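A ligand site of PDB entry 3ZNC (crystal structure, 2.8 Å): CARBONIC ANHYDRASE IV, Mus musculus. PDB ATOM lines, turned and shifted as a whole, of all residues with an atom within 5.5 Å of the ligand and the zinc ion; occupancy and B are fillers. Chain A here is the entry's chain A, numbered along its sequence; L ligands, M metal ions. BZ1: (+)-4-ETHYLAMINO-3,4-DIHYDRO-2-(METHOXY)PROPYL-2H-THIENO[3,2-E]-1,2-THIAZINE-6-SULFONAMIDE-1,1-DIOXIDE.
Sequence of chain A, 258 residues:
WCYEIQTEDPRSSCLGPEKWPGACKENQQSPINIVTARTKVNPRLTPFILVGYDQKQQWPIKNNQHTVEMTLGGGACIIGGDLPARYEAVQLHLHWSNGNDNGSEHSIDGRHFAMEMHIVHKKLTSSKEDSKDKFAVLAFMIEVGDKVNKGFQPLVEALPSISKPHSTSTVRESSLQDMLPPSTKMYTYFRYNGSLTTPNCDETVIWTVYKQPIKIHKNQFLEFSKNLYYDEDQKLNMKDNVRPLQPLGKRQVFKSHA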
ATOM      1  N   TRP A   1     -21.206  12.839  -4.857  1.00  0.00           N
ATOM      2  CA  TRP A   1     -20.247  13.529  -5.776  1.00  0.00           C
ATOM      3  C   TRP A   1     -21.023  14.605  -6.525  1.00  0.00           C
ATOM      4  O   TRP A   1     -22.253  14.530  -6.625  1.00  0.00           O
ATOM      5  CB  TRP A   1     -19.600  12.503  -6.794  1.00  0.00           C
ATOM      6  CG  TRP A   1     -20.545  11.927  -7.830  1.00  0.00           C
ATOM      7  CD1 TRP A   1     -21.179  10.717  -7.785  1.00  0.00           C
ATOM      8  CD2 TRP A   1     -20.916  12.527  -9.087  1.00  0.00           C
ATOM      9  NE1 TRP A   1     -21.917  10.518  -8.938  1.00  0.00           N
ATOM     10  CE2 TRP A   1     -21.771  11.608  -9.748  1.00  0.00           C
ATOM     11  CE3 TRP A   1     -20.602  13.736  -9.714  1.00  0.00           C
ATOM     12  CZ2 TRP A   1     -22.321  11.881 -10.999  1.00  0.00           C
ATOM     13  CZ3 TRP A   1     -21.152  14.009 -10.965  1.00  0.00           C
ATOM     14  CH2 TRP A   1     -22.002  13.077 -11.597  1.00  0.00           C
ATOM     15  N   ASN A  64     -32.055  13.086 -13.469  1.00  0.00           N
ATOM     16  CA  ASN A  64     -31.356  12.183 -12.557  1.00  0.00           C
ATOM     17  C   ASN A  64     -30.472  12.883 -11.540  1.00  0.00           C
ATOM     18  O   ASN A  64     -29.686  12.231 -10.854  1.00  0.00           O
ATOM     19  CB  ASN A  64     -30.525  11.103 -13.355  1.00  0.00           C
ATOM     20  CG  ASN A  64     -29.411  11.708 -14.187  1.00  0.00           C
ATOM     21  OD1 ASN A  64     -29.041  12.871 -14.018  1.00  0.00           O
ATOM     22  ND2 ASN A  64     -28.857  10.907 -15.092  1.00  0.00           N
ATOM     23  N   HIS A  66     -28.174  15.007 -12.314  1.00  0.00           N
ATOM     24  CA  HIS A  66     -26.917  15.381 -12.958  1.00  0.00           C
ATOM     25  C   HIS A  66     -27.151  15.810 -14.404  1.00  0.00           C
ATOM     26  O   HIS A  66     -26.321  16.513 -14.993  1.00  0.00           O
ATOM     27  CB  HIS A  66     -25.890  14.207 -12.917  1.00  0.00           C
ATOM     28  CG  HIS A  66     -25.632  13.677 -11.531  1.00  0.00           C
ATOM     29  ND1 HIS A  66     -25.051  14.436 -10.538  1.00  0.00           N
ATOM     30  CD2 HIS A  66     -25.888  12.471 -10.971  1.00  0.00           C
ATOM     31  CE1 HIS A  66     -24.953  13.721  -9.432  1.00  0.00           C
ATOM     32  NE2 HIS A  66     -25.461  12.524  -9.671  1.00  0.00           N
ATOM     33  N   THR A  67     -28.282  15.413 -14.966  1.00  0.00           N
ATOM     34  CA  THR A  67     -28.608  15.739 -16.351  1.00  0.00           C
ATOM     35  C   THR A  67     -30.027  15.272 -16.644  1.00  0.00           C
ATOM     36  O   THR A  67     -30.732  14.775 -15.754  1.00  0.00           O
ATOM     37  CB  THR A  67     -27.601  15.067 -17.302  1.00  0.00           C
ATOM     38  OG1 THR A  67     -27.889  15.409 -18.659  1.00  0.00           O
ATOM     39  CG2 THR A  67     -27.636  13.548 -17.140  1.00  0.00           C
ATOM     40  N   GLU A  69     -32.047  12.661 -18.384  1.00  0.00           N
ATOM     41  CA  GLU A  69     -31.897  11.315 -18.918  1.00  0.00           C
ATOM     42  C   GLU A  69     -33.131  10.880 -19.712  1.00  0.00           C
ATOM     43  O   GLU A  69     -34.258  11.062 -19.276  1.00  0.00           O
ATOM     44  CB  GLU A  69     -31.620  10.324 -17.732  1.00  0.00           C
ATOM     45  CG  GLU A  69     -31.161   8.937 -18.145  1.00  0.00           C
ATOM     46  CD  GLU A  69     -30.899   8.030 -16.953  1.00  0.00           C
ATOM     47  OE1 GLU A  69     -30.792   8.532 -15.809  1.00  0.00           O
ATOM     48  OE2 GLU A  69     -30.799   6.790 -17.150  1.00  0.00           O
ATOM     49  N   VAL A  90     -29.183   2.564 -24.922  1.00  0.00           N
ATOM     50  CA  VAL A  90     -29.689   2.447 -23.553  1.00  0.00           C
ATOM     51  C   VAL A  90     -30.305   3.757 -23.047  1.00  0.00           C
ATOM     52  O   VAL A  90     -31.456   3.783 -22.626  1.00  0.00           O
ATOM     53  CB  VAL A  90     -28.585   1.944 -22.582  1.00  0.00           C
ATOM     54  CG1 VAL A  90     -28.823   2.451 -21.158  1.00  0.00           C
ATOM     55  CG2 VAL A  90     -28.544   0.426 -22.576  1.00  0.00           C
ATOM     56  N   GLN A  91     -29.543   4.856 -23.114  1.00  0.00           N
ATOM     57  CA  GLN A  91     -30.010   6.157 -22.648  1.00  0.00           C
ATOM     58  C   GLN A  91     -29.421   7.289 -23.484  1.00  0.00           C
ATOM     59  O   GLN A  91     -28.514   7.088 -24.281  1.00  0.00           O
ATOM     60  CB  GLN A  91     -29.603   6.375 -21.161  1.00  0.00           C
ATOM     61  CG  GLN A  91     -28.145   6.734 -20.990  1.00  0.00           C
ATOM     62  CD  GLN A  91     -27.851   7.363 -19.649  1.00  0.00           C
ATOM     63  OE1 GLN A  91     -27.347   8.481 -19.571  1.00  0.00           O
ATOM     64  NE2 GLN A  91     -28.198   6.662 -18.587  1.00  0.00           N
ATOM     65  N   HIS A  93     -28.485  11.656 -22.874  1.00  0.00           N
ATOM     66  CA  HIS A  93     -28.465  12.809 -21.988  1.00  0.00           C
ATOM     67  C   HIS A  93     -27.616  13.909 -22.603  1.00  0.00           C
ATOM     68  O   HIS A  93     -27.067  13.729 -23.693  1.00  0.00           O
ATOM     69  CB  HIS A  93     -27.939  12.416 -20.560  1.00  0.00           C
ATOM     70  CG  HIS A  93     -26.512  11.956 -20.537  1.00  0.00           C
ATOM     71  ND1 HIS A  93     -26.130  10.641 -20.459  1.00  0.00           N
ATOM     72  CD2 HIS A  93     -25.369  12.670 -20.563  1.00  0.00           C
ATOM     73  CE1 HIS A  93     -24.792  10.597 -20.437  1.00  0.00           C
ATOM     74  NE2 HIS A  93     -24.279  11.811 -20.501  1.00  0.00           N
ATOM     75  N   HIS A  95     -24.972  17.691 -21.748  1.00  0.00           N
ATOM     76  CA  HIS A  95     -24.103  18.487 -20.856  1.00  0.00           C
ATOM     77  C   HIS A  95     -24.102  19.921 -21.399  1.00  0.00           C
ATOM     78  O   HIS A  95     -23.858  20.137 -22.584  1.00  0.00           O
ATOM     79  CB  HIS A  95     -22.625  17.944 -20.847  1.00  0.00           C
ATOM     80  CG  HIS A  95     -22.528  16.520 -20.416  1.00  0.00           C
ATOM     81  ND1 HIS A  95     -22.185  16.123 -19.138  1.00  0.00           N
ATOM     82  CD2 HIS A  95     -22.737  15.375 -21.112  1.00  0.00           C
ATOM     83  CE1 HIS A  95     -22.213  14.784 -19.100  1.00  0.00           C
ATOM     84  NE2 HIS A  95     -22.540  14.284 -20.272  1.00  0.00           N
ATOM     85  N   GLU A 105     -18.254  19.073 -23.207  1.00  0.00           N
ATOM     86  CA  GLU A 105     -17.146  18.495 -22.478  1.00  0.00           C
ATOM     87  C   GLU A 105     -15.918  18.395 -23.380  1.00  0.00           C
ATOM     88  O   GLU A 105     -14.861  18.936 -23.060  1.00  0.00           O
ATOM     89  CB  GLU A 105     -17.546  17.096 -21.899  1.00  0.00           C
ATOM     90  CG  GLU A 105     -18.666  17.199 -20.875  1.00  0.00           C
ATOM     91  CD  GLU A 105     -18.876  15.931 -20.077  1.00  0.00           C
ATOM     92  OE1 GLU A 105     -19.222  14.893 -20.669  1.00  0.00           O
ATOM     93  OE2 GLU A 105     -18.708  15.986 -18.840  1.00  0.00           O
ATOM     94  N   HIS A 118     -25.014  12.924 -25.549  1.00  0.00           N
ATOM     95  CA  HIS A 118     -24.431  11.612 -25.412  1.00  0.00           C
ATOM     96  C   HIS A 118     -25.428  10.469 -25.487  1.00  0.00           C
ATOM     97  O   HIS A 118     -26.258  10.300 -24.598  1.00  0.00           O
ATOM     98  CB  HIS A 118     -23.608  11.513 -24.080  1.00  0.00           C
ATOM     99  CG  HIS A 118     -22.351  12.319 -24.097  1.00  0.00           C
ATOM    100  ND1 HIS A 118     -21.799  12.829 -22.945  1.00  0.00           N
ATOM    101  CD2 HIS A 118     -21.556  12.646 -25.149  1.00  0.00           C
ATOM    102  CE1 HIS A 118     -20.691  13.436 -23.315  1.00  0.00           C
ATOM    103  NE2 HIS A 118     -20.496  13.348 -24.641  1.00  0.00           N
ATOM    104  N   VAL A 120     -25.687   6.747 -25.211  1.00  0.00           N
ATOM    105  CA  VAL A 120     -24.967   5.594 -24.680  1.00  0.00           C
ATOM    106  C   VAL A 120     -25.453   4.244 -25.196  1.00  0.00           C
ATOM    107  O   VAL A 120     -26.655   3.995 -25.240  1.00  0.00           O
ATOM    108  CB  VAL A 120     -25.020   5.584 -23.136  1.00  0.00           C
ATOM    109  CG1 VAL A 120     -24.057   4.549 -22.569  1.00  0.00           C
ATOM    110  CG2 VAL A 120     -24.700   6.955 -22.588  1.00  0.00           C
ATOM    111  N   LYS A 122     -24.784  -0.018 -24.774  1.00  0.00           N
ATOM    112  CA  LYS A 122     -24.146  -1.099 -24.018  1.00  0.00           C
ATOM    113  C   LYS A 122     -23.777  -2.229 -24.989  1.00  0.00           C
ATOM    114  O   LYS A 122     -24.534  -2.530 -25.909  1.00  0.00           O
ATOM    115  CB  LYS A 122     -25.128  -1.646 -22.916  1.00  0.00           C
ATOM    116  CG  LYS A 122     -24.662  -2.916 -22.215  1.00  0.00           C
ATOM    117  CD  LYS A 122     -25.837  -3.649 -21.539  1.00  0.00           C
ATOM    118  CE  LYS A 122     -26.378  -2.892 -20.324  1.00  0.00           C
ATOM    119  NZ  LYS A 122     -25.405  -2.845 -19.184  1.00  0.00           N
ATOM    120  N   PHE A 135     -18.962   0.034 -23.660  1.00  0.00           N
ATOM    121  CA  PHE A 135     -19.846   1.155 -23.925  1.00  0.00           C
ATOM    122  C   PHE A 135     -19.399   1.845 -25.206  1.00  0.00           C
ATOM    123  O   PHE A 135     -18.214   2.042 -25.432  1.00  0.00           O
ATOM    124  CB  PHE A 135     -19.804   2.173 -22.748  1.00  0.00           C
ATOM    125  CG  PHE A 135     -20.645   1.787 -21.589  1.00  0.00           C
ATOM    126  CD1 PHE A 135     -22.027   1.725 -21.710  1.00  0.00           C
ATOM    127  CD2 PHE A 135     -20.075   1.494 -20.361  1.00  0.00           C
ATOM    128  CE1 PHE A 135     -22.831   1.382 -20.621  1.00  0.00           C
ATOM    129  CE2 PHE A 135     -20.857   1.147 -19.271  1.00  0.00           C
ATOM    130  CZ  PHE A 135     -22.240   1.100 -19.399  1.00  0.00           C
ATOM    131  N   VAL A 137     -20.242   5.255 -26.885  1.00  0.00           N
ATOM    132  CA  VAL A 137     -20.936   6.518 -26.693  1.00  0.00           C
ATOM    133  C   VAL A 137     -20.746   7.411 -27.911  1.00  0.00           C
ATOM    134  O   VAL A 137     -19.613   7.675 -28.332  1.00  0.00           O
ATOM    135  CB  VAL A 137     -20.422   7.260 -25.422  1.00  0.00           C
ATOM    136  CG1 VAL A 137     -21.125   8.620 -25.281  1.00  0.00           C
ATOM    137  CG2 VAL A 137     -20.665   6.411 -24.178  1.00  0.00           C
ATOM    138  N   SER A 195     -13.210   6.872 -21.112  1.00  0.00           N
ATOM    139  CA  SER A 195     -14.047   6.478 -19.985  1.00  0.00           C
ATOM    140  C   SER A 195     -15.316   7.304 -19.824  1.00  0.00           C
ATOM    141  O   SER A 195     -15.547   8.268 -20.570  1.00  0.00           O
ATOM    142  CB  SER A 195     -13.212   6.625 -18.661  1.00  0.00           C
ATOM    143  OG  SER A 195     -12.753   7.970 -18.517  1.00  0.00           O
ATOM    144  N   LEU A 196     -16.148   6.915 -18.860  1.00  0.00           N
ATOM    145  CA  LEU A 196     -17.360   7.667 -18.534  1.00  0.00           C
ATOM    146  C   LEU A 196     -16.843   9.009 -18.027  1.00  0.00           C
ATOM    147  O   LEU A 196     -15.799   9.061 -17.362  1.00  0.00           O
ATOM    148  CB  LEU A 196     -18.139   6.966 -17.356  1.00  0.00           C
ATOM    149  CG  LEU A 196     -19.154   5.792 -17.551  1.00  0.00           C
ATOM    150  CD1 LEU A 196     -18.635   4.751 -18.501  1.00  0.00           C
ATOM    151  CD2 LEU A 196     -19.439   5.170 -16.201  1.00  0.00           C
ATOM    152  N   THR A 197     -17.561  10.088 -18.297  1.00  0.00           N
ATOM    153  CA  THR A 197     -17.139  11.406 -17.865  1.00  0.00           C
ATOM    154  C   THR A 197     -17.641  11.781 -16.462  1.00  0.00           C
ATOM    155  O   THR A 197     -17.465  12.901 -16.000  1.00  0.00           O
ATOM    156  CB  THR A 197     -17.534  12.476 -18.890  1.00  0.00           C
ATOM    157  OG1 THR A 197     -18.948  12.463 -19.105  1.00  0.00           O
ATOM    158  CG2 THR A 197     -16.817  12.226 -20.206  1.00  0.00           C
ATOM    159  N   THR A 198     -18.289  10.824 -15.789  1.00  0.00           N
ATOM    160  CA  THR A 198     -18.811  11.001 -14.440  1.00  0.00           C
ATOM    161  C   THR A 198     -18.337   9.787 -13.645  1.00  0.00           C
ATOM    162  O   THR A 198     -17.939   8.784 -14.238  1.00  0.00           O
ATOM    163  CB  THR A 198     -20.364  11.048 -14.419  1.00  0.00           C
ATOM    164  OG1 THR A 198     -20.894   9.829 -14.932  1.00  0.00           O
ATOM    165  CG2 THR A 198     -20.883  12.203 -15.251  1.00  0.00           C
ATOM    166  N   PRO A 199     -18.358   9.858 -12.297  1.00  0.00           N
ATOM    167  CA  PRO A 199     -17.919   8.716 -11.489  1.00  0.00           C
ATOM    168  C   PRO A 199     -18.748   7.469 -11.808  1.00  0.00           C
ATOM    169  O   PRO A 199     -19.917   7.579 -12.192  1.00  0.00           O
ATOM    170  CB  PRO A 199     -18.168   9.218 -10.017  1.00  0.00           C
ATOM    171  CG  PRO A 199     -17.976  10.679 -10.148  1.00  0.00           C
ATOM    172  CD  PRO A 199     -18.716  10.998 -11.436  1.00  0.00           C
ATOM    173  N   TRP A 207     -15.270   5.944 -27.657  1.00  0.00           N
ATOM    174  CA  TRP A 207     -15.882   7.222 -28.050  1.00  0.00           C
ATOM    175  C   TRP A 207     -15.872   7.548 -29.529  1.00  0.00           C
ATOM    176  O   TRP A 207     -14.875   7.327 -30.220  1.00  0.00           O
ATOM    177  CB  TRP A 207     -15.214   8.425 -27.293  1.00  0.00           C
ATOM    178  CG  TRP A 207     -15.578   8.539 -25.852  1.00  0.00           C
ATOM    179  CD1 TRP A 207     -14.931   7.951 -24.804  1.00  0.00           C
ATOM    180  CD2 TRP A 207     -16.672   9.281 -25.293  1.00  0.00           C
ATOM    181  NE1 TRP A 207     -15.559   8.289 -23.625  1.00  0.00           N
ATOM    182  CE2 TRP A 207     -16.623   9.100 -23.901  1.00  0.00           C
ATOM    183  CE3 TRP A 207     -17.684  10.069 -25.846  1.00  0.00           C
ATOM    184  CZ2 TRP A 207     -17.551   9.703 -23.039  1.00  0.00           C
ATOM    185  CZ3 TRP A 207     -18.604  10.668 -24.995  1.00  0.00           C
ATOM    186  CH2 TRP A 207     -18.538  10.476 -23.604  1.00  0.00           C
HETATM  187  C3  BZ1 L   1     -23.202   3.062 -14.840  1.00  0.00           C
HETATM  188  C9  BZ1 L   1     -22.821   7.721 -17.090  1.00  0.00           C
HETATM  189  C10 BZ1 L   1     -23.242   6.731 -18.211  1.00  0.00           C
HETATM  190  C11 BZ1 L   1     -23.197   7.481 -15.613  1.00  0.00           C
HETATM  191  C12 BZ1 L   1     -24.295   6.404 -15.487  1.00  0.00           C
HETATM  192  S1  BZ1 L   1     -21.187   9.693 -20.067  1.00  0.00           S
HETATM  193  C4  BZ1 L   1     -22.620   1.802 -15.483  1.00  0.00           C
HETATM  194  C5  BZ1 L   1     -24.878  10.403 -16.093  1.00  0.00           C
HETATM  195  C6  BZ1 L   1     -25.107   9.185 -15.194  1.00  0.00           C
HETATM  196  S2  BZ1 L   1     -22.614   7.203 -19.811  1.00  0.00           S
HETATM  197  N2  BZ1 L   1     -21.378  11.262 -19.551  1.00  0.00           N
HETATM  198  O3  BZ1 L   1     -19.603   9.575 -20.183  1.00  0.00           O
HETATM  199  O4  BZ1 L   1     -21.975   9.599 -21.427  1.00  0.00           O
HETATM  200  C7  BZ1 L   1     -21.999   8.617 -18.951  1.00  0.00           C
HETATM  201  C8  BZ1 L   1     -22.155   8.743 -17.634  1.00  0.00           C
HETATM  202  S3  BZ1 L   1     -24.185   5.253 -17.809  1.00  0.00           S
HETATM  203  O2  BZ1 L   1     -23.558   3.998 -18.539  1.00  0.00           O
HETATM  204  O5  BZ1 L   1     -25.730   5.368 -18.193  1.00  0.00           O
HETATM  205  N3  BZ1 L   1     -24.034   5.067 -16.112  1.00  0.00           N
HETATM  206  N1  BZ1 L   1     -23.760   8.649 -14.825  1.00  0.00           N
HETATM  207  C2  BZ1 L   1     -22.852   4.287 -15.666  1.00  0.00           C
HETATM  208  O1  BZ1 L   1     -23.690   0.981 -15.987  1.00  0.00           O
HETATM  209  C1  BZ1 L   1     -24.628   0.323 -15.100  1.00  0.00           C
HETATM  210 ZN    ZN M   1     -22.352  12.311 -20.825  1.00  0.00          ZN
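An oxygen (O3) of the ligand sits at hydrogen-bond distance from the backbone NH (N) of Thr 197 (2.8 Å).
The side-chain amide nitrogen of Gln 91 is in hydrogen-bond range of an oxygen (O5) of the ligand, 2.8 Å away.
OG1 of Thr 198 is in hydrogen-bond range of N1 of the ligand (3.1 Å).
The side-chain hydroxyl of Thr 197 sits at hydrogen-bond distance from an oxygen (O3) of the ligand (3.2 Å).
N of Val 90 lies within hydrogen-bond range of O of Val 120 (2.9 Å).
O of Gln 91 lies within hydrogen-bond range of N of Val 120.
The backbone carbonyl oxygen (O) of Ser 195 sits at hydrogen-bond distance from the indole nitrogen (NE1) of Trp 207, at 3.1 Å.
A ring nitrogen (ND1) of His 95 sits close to the side-chain carboxylate (OE2) of Glu 105 (3.5 Å).
The side-chain carboxylate of Glu 105 is in hydrogen-bond range of the side-chain hydroxyl of Thr 197 (2.9 Å).
The side-chain amide oxygen (OE1) of Gln 91 lies within hydrogen-bond range of a ring nitrogen (ND1) of His 93 (2.6 Å).
The side-chain amide nitrogen of Gln 91 is in hydrogen-bond range of the side-chain carboxylate of Glu 69, 3.0 Å away.
Val 120 touches the ligand (CG2 to S2, 3.5 Å).
Phe 135 touches the ligand (CZ to O2, 3.3 Å).
Leu 196 touches the ligand.
Trp 207 touches the ligand.
Merely in contact with the zinc ion: Thr 197 (3.8 Å).
The zinc ion is bound by a nitrogen (N2) of the ligand (1.9 Å), a ring nitrogen (NE2) of His 93 (2.0 Å), a ring nitrogen (NE2) of His 95 (2.1 Å) and a ring nitrogen (ND1) of His 118 (2.3 Å).
Slightly farther from the zinc ion lies an oxygen (O4) of the ligand (2.8 Å).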
